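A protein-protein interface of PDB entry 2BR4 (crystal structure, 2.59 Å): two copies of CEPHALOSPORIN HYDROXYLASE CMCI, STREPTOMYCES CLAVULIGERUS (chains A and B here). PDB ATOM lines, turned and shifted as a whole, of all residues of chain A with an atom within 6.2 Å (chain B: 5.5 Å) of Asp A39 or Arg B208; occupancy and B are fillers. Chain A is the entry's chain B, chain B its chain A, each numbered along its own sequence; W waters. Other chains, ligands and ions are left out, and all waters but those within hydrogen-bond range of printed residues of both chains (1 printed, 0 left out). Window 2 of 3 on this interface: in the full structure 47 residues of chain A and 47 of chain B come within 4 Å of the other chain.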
ATOM      1  N   PRO A  37     -13.467 -21.140  23.798  1.00  0.00           N
ATOM      2  CA  PRO A  37     -12.784 -21.010  25.089  1.00  0.00           C
ATOM      3  C   PRO A  37     -12.803 -19.558  25.562  1.00  0.00           C
ATOM      4  O   PRO A  37     -12.594 -18.649  24.758  1.00  0.00           O
ATOM      5  CB  PRO A  37     -11.351 -21.461  24.778  1.00  0.00           C
ATOM      6  CG  PRO A  37     -11.174 -21.150  23.329  1.00  0.00           C
ATOM      7  CD  PRO A  37     -12.516 -21.421  22.708  1.00  0.00           C
ATOM      8  N   LEU A  38     -13.046 -19.348  26.849  1.00  0.00           N
ATOM      9  CA  LEU A  38     -13.250 -18.003  27.382  1.00  0.00           C
ATOM     10  C   LEU A  38     -11.939 -17.208  27.496  1.00  0.00           C
ATOM     11  O   LEU A  38     -11.955 -15.984  27.414  1.00  0.00           O
ATOM     12  CB  LEU A  38     -13.978 -18.070  28.730  1.00  0.00           C
ATOM     13  CG  LEU A  38     -15.496 -17.838  28.719  1.00  0.00           C
ATOM     14  CD1 LEU A  38     -16.184 -18.508  27.564  1.00  0.00           C
ATOM     15  CD2 LEU A  38     -16.099 -18.303  30.043  1.00  0.00           C
ATOM     16  N   ASP A  39     -10.812 -17.899  27.666  1.00  0.00           N
ATOM     17  CA  ASP A  39      -9.499 -17.237  27.656  1.00  0.00           C
ATOM     18  C   ASP A  39      -9.184 -16.581  26.298  1.00  0.00           C
ATOM     19  O   ASP A  39      -8.283 -15.751  26.207  1.00  0.00           O
ATOM     20  CB  ASP A  39      -8.363 -18.197  28.070  1.00  0.00           C
ATOM     21  CG  ASP A  39      -8.119 -19.302  27.053  1.00  0.00           C
ATOM     22  OD1 ASP A  39      -8.946 -20.226  26.977  1.00  0.00           O
ATOM     23  OD2 ASP A  39      -7.139 -19.344  26.284  1.00  0.00           O
ATOM     24  N   ARG A  40      -9.928 -16.954  25.256  1.00  0.00           N
ATOM     25  CA  ARG A  40      -9.780 -16.343  23.936  1.00  0.00           C
ATOM     26  C   ARG A  40     -11.080 -15.695  23.493  1.00  0.00           C
ATOM     27  O   ARG A  40     -11.388 -15.655  22.310  1.00  0.00           O
ATOM     28  CB  ARG A  40      -9.358 -17.388  22.903  1.00  0.00           C
ATOM     29  CG  ARG A  40      -8.099 -18.178  23.260  1.00  0.00           C
ATOM     30  CD  ARG A  40      -7.088 -18.291  22.135  1.00  0.00           C
ATOM     31  NE  ARG A  40      -7.712 -18.516  20.824  1.00  0.00           N
ATOM     32  CZ  ARG A  40      -7.055 -18.869  19.722  1.00  0.00           C
ATOM     33  NH1 ARG A  40      -5.733 -19.044  19.741  1.00  0.00           N
ATOM     34  NH2 ARG A  40      -7.722 -19.051  18.593  1.00  0.00           N
ATOM     35  N   TRP A  41     -11.834 -15.165  24.446  1.00  0.00           N
ATOM     36  CA  TRP A  41     -13.156 -14.606  24.153  1.00  0.00           C
ATOM     37  C   TRP A  41     -13.113 -13.510  23.085  1.00  0.00           C
ATOM     38  O   TRP A  41     -13.993 -13.436  22.246  1.00  0.00           O
ATOM     39  CB  TRP A  41     -13.768 -14.053  25.432  1.00  0.00           C
ATOM     40  CG  TRP A  41     -15.036 -13.319  25.242  1.00  0.00           C
ATOM     41  CD1 TRP A  41     -16.295 -13.835  25.297  1.00  0.00           C
ATOM     42  CD2 TRP A  41     -15.186 -11.921  24.997  1.00  0.00           C
ATOM     43  NE1 TRP A  41     -17.222 -12.844  25.094  1.00  0.00           N
ATOM     44  CE2 TRP A  41     -16.569 -11.657  24.904  1.00  0.00           C
ATOM     45  CE3 TRP A  41     -14.290 -10.861  24.834  1.00  0.00           C
ATOM     46  CZ2 TRP A  41     -17.076 -10.381  24.659  1.00  0.00           C
ATOM     47  CZ3 TRP A  41     -14.795  -9.592  24.592  1.00  0.00           C
ATOM     48  CH2 TRP A  41     -16.178  -9.362  24.507  1.00  0.00           C
ATOM     49  N   ALA A  42     -12.078 -12.677  23.126  1.00  0.00           N
ATOM     50  CA  ALA A  42     -11.973 -11.502  22.261  1.00  0.00           C
ATOM     51  C   ALA A  42     -11.671 -11.831  20.804  1.00  0.00           C
ATOM     52  O   ALA A  42     -11.939 -11.018  19.930  1.00  0.00           O
ATOM     53  CB  ALA A  42     -10.914 -10.554  22.804  1.00  0.00           C
ATOM     54  N   GLU A  43     -11.113 -13.015  20.553  1.00  0.00           N
ATOM     55  CA  GLU A  43     -10.754 -13.458  19.200  1.00  0.00           C
ATOM     56  C   GLU A  43     -11.857 -14.254  18.498  1.00  0.00           C
ATOM     57  O   GLU A  43     -11.639 -14.793  17.409  1.00  0.00           O
ATOM     58  CB  GLU A  43      -9.486 -14.316  19.261  1.00  0.00           C
ATOM     59  CG  GLU A  43      -8.273 -13.574  19.816  1.00  0.00           C
ATOM     60  CD  GLU A  43      -7.115 -14.487  20.169  1.00  0.00           C
ATOM     61  OE1 GLU A  43      -6.005 -13.951  20.380  1.00  0.00           O
ATOM     62  OE2 GLU A  43      -7.300 -15.729  20.249  1.00  0.00           O
ATOM     63  N   LEU B 204     -13.451 -12.957  32.672  1.00  0.00           N
ATOM     64  CA  LEU B 204     -14.045 -13.987  31.825  1.00  0.00           C
ATOM     65  C   LEU B 204     -13.094 -15.168  31.630  1.00  0.00           C
ATOM     66  O   LEU B 204     -13.525 -16.316  31.601  1.00  0.00           O
ATOM     67  CB  LEU B 204     -14.431 -13.425  30.450  1.00  0.00           C
ATOM     68  CG  LEU B 204     -15.902 -13.460  30.013  1.00  0.00           C
ATOM     69  CD1 LEU B 204     -15.977 -13.283  28.500  1.00  0.00           C
ATOM     70  CD2 LEU B 204     -16.652 -14.729  30.422  1.00  0.00           C
ATOM     71  N   GLY B 205     -11.804 -14.883  31.503  1.00  0.00           N
ATOM     72  CA  GLY B 205     -10.797 -15.916  31.307  1.00  0.00           C
ATOM     73  C   GLY B 205     -10.552 -16.788  32.530  1.00  0.00           C
ATOM     74  O   GLY B 205     -10.052 -17.905  32.412  1.00  0.00           O
ATOM     75  N   ALA B 206     -10.902 -16.277  33.709  1.00  0.00           N
ATOM     76  CA  ALA B 206     -10.798 -17.035  34.953  1.00  0.00           C
ATOM     77  C   ALA B 206     -11.786 -18.202  34.995  1.00  0.00           C
ATOM     78  O   ALA B 206     -11.609 -19.137  35.774  1.00  0.00           O
ATOM     79  CB  ALA B 206     -11.022 -16.121  36.133  1.00  0.00           C
ATOM     80  N   PHE B 207     -12.822 -18.136  34.153  1.00  0.00           N
ATOM     81  CA  PHE B 207     -13.800 -19.214  34.010  1.00  0.00           C
ATOM     82  C   PHE B 207     -13.533 -20.147  32.816  1.00  0.00           C
ATOM     83  O   PHE B 207     -14.432 -20.865  32.395  1.00  0.00           O
ATOM     84  CB  PHE B 207     -15.205 -18.619  33.857  1.00  0.00           C
ATOM     85  CG  PHE B 207     -15.711 -17.915  35.075  1.00  0.00           C
ATOM     86  CD1 PHE B 207     -15.301 -16.626  35.367  1.00  0.00           C
ATOM     87  CD2 PHE B 207     -16.622 -18.530  35.911  1.00  0.00           C
ATOM     88  CE1 PHE B 207     -15.785 -15.961  36.490  1.00  0.00           C
ATOM     89  CE2 PHE B 207     -17.104 -17.879  37.033  1.00  0.00           C
ATOM     90  CZ  PHE B 207     -16.689 -16.590  37.325  1.00  0.00           C
ATOM     91  N   ARG B 208     -12.311 -20.162  32.284  1.00  0.00           N
ATOM     92  CA  ARG B 208     -12.006 -20.942  31.071  1.00  0.00           C
ATOM     93  C   ARG B 208     -12.225 -22.458  31.176  1.00  0.00           C
ATOM     94  O   ARG B 208     -12.580 -23.100  30.198  1.00  0.00           O
ATOM     95  CB  ARG B 208     -10.575 -20.667  30.595  1.00  0.00           C
ATOM     96  CG  ARG B 208      -9.455 -21.141  31.526  1.00  0.00           C
ATOM     97  CD  ARG B 208      -8.090 -20.560  31.177  1.00  0.00           C
ATOM     98  NE  ARG B 208      -7.387 -20.075  32.364  1.00  0.00           N
ATOM     99  CZ  ARG B 208      -6.540 -20.799  33.100  1.00  0.00           C
ATOM    100  NH1 ARG B 208      -6.266 -22.062  32.780  1.00  0.00           N
ATOM    101  NH2 ARG B 208      -5.957 -20.260  34.168  1.00  0.00           N
ATOM    102  N   ASP B 209     -12.007 -23.022  32.357  1.00  0.00           N
ATOM    103  CA  ASP B 209     -12.138 -24.461  32.574  1.00  0.00           C
ATOM    104  C   ASP B 209     -13.542 -24.917  32.955  1.00  0.00           C
ATOM    105  O   ASP B 209     -13.788 -26.121  33.043  1.00  0.00           O
ATOM    106  CB  ASP B 209     -11.167 -24.914  33.669  1.00  0.00           C
ATOM    107  CG  ASP B 209      -9.717 -24.664  33.309  1.00  0.00           C
ATOM    108  OD1 ASP B 209      -9.375 -24.815  32.116  1.00  0.00           O
ATOM    109  OD2 ASP B 209      -8.846 -24.319  34.145  1.00  0.00           O
ATOM    110  N   VAL B 210     -14.458 -23.975  33.190  1.00  0.00           N
ATOM    111  CA  VAL B 210     -15.813 -24.316  33.646  1.00  0.00           C
ATOM    112  C   VAL B 210     -16.931 -23.849  32.718  1.00  0.00           C
ATOM    113  O   VAL B 210     -17.944 -24.529  32.600  1.00  0.00           O
ATOM    114  CB  VAL B 210     -16.087 -23.806  35.077  1.00  0.00           C
ATOM    115  CG1 VAL B 210     -15.207 -24.536  36.070  1.00  0.00           C
ATOM    116  CG2 VAL B 210     -15.869 -22.305  35.186  1.00  0.00           C
ATOM    117  N   LEU B 211     -16.767 -22.698  32.073  1.00  0.00           N
ATOM    118  CA  LEU B 211     -17.753 -22.205  31.105  1.00  0.00           C
ATOM    119  C   LEU B 211     -17.138 -21.997  29.726  1.00  0.00           C
ATOM    120  O   LEU B 211     -15.956 -21.684  29.614  1.00  0.00           O
ATOM    121  CB  LEU B 211     -18.373 -20.899  31.591  1.00  0.00           C
ATOM    122  CG  LEU B 211     -19.093 -21.008  32.935  1.00  0.00           C
ATOM    123  CD1 LEU B 211     -19.346 -19.617  33.514  1.00  0.00           C
ATOM    124  CD2 LEU B 211     -20.397 -21.793  32.799  1.00  0.00           C
ATOM    125  N   VAL B 232     -19.208 -26.521  30.757  1.00  0.00           N
ATOM    126  CA  VAL B 232     -18.500 -27.591  30.048  1.00  0.00           C
ATOM    127  C   VAL B 232     -18.223 -28.773  30.983  1.00  0.00           C
ATOM    128  O   VAL B 232     -18.286 -28.636  32.206  1.00  0.00           O
ATOM    129  CB  VAL B 232     -17.154 -27.103  29.459  1.00  0.00           C
ATOM    130  CG1 VAL B 232     -17.344 -25.847  28.637  1.00  0.00           C
ATOM    131  CG2 VAL B 232     -16.112 -26.873  30.567  1.00  0.00           C
HETATM  132  O   HOH W   1     -13.789 -21.820  28.314  1.00  0.00           O
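The guanidinium group (NE) of Arg B208 sits close to the backbone carbonyl oxygen (O) of Gly B205, at 3.4 Å. NH1 of Arg B208 is in salt-bridge range of OD2 of Asp B209 (3.7 Å).
O of Leu B204 touches CB of Leu A38, at 3.4 Å. Leu A38 touches Phe B207 (CD2 to O, 3.9 Å). CD2 of Leu A38 touches O of Leu B211 (3.4 Å). CB of Asp A39 touches CD of Arg B208, 3.9 Å away. Leu B204 touches Trp A41 (CD1 to CD1, 3.3 Å).
Of chain B, only Arg B208 (3.9 Å) comes within 4 Å of Asp A39. Of the printed residues of chain B, Trp A41 touches Leu B204. Of the printed residues of chain A, Leu B204 touches Leu A38 (3.4 Å) and Trp A41 (3.3 Å). Of the printed residues of chain A, Phe B207 touches Leu A38 (3.9 Å). Arg B208 touches just one residue of chain A: Asp A39. Printed residues of chain A within 4 Å of Leu B211: Leu A38 (3.4 Å). The nearest residue of chain B that does not touch Asp A39 is Gly B205 (4.1 Å).
Of the 7 printed residues of chain A, 3 touch a printed residue of chain B. Printed residues of chain A that touch a printed residue of chain B: Leu A38, Asp A39 and Trp A41. Hydrophobic or aromatic side chains of chain A within 4 Å of the printed part of chain B: Leu A38 and Trp A41. Among the printed residues, 5 pairs touch across the chains.
No position is printed for both chains.
Water W1 lies within hydrogen-bond range of O of Leu B211 (2.5 Å), O of Arg B208 (2.6 Å) and N of Leu A38 (3.0 Å).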
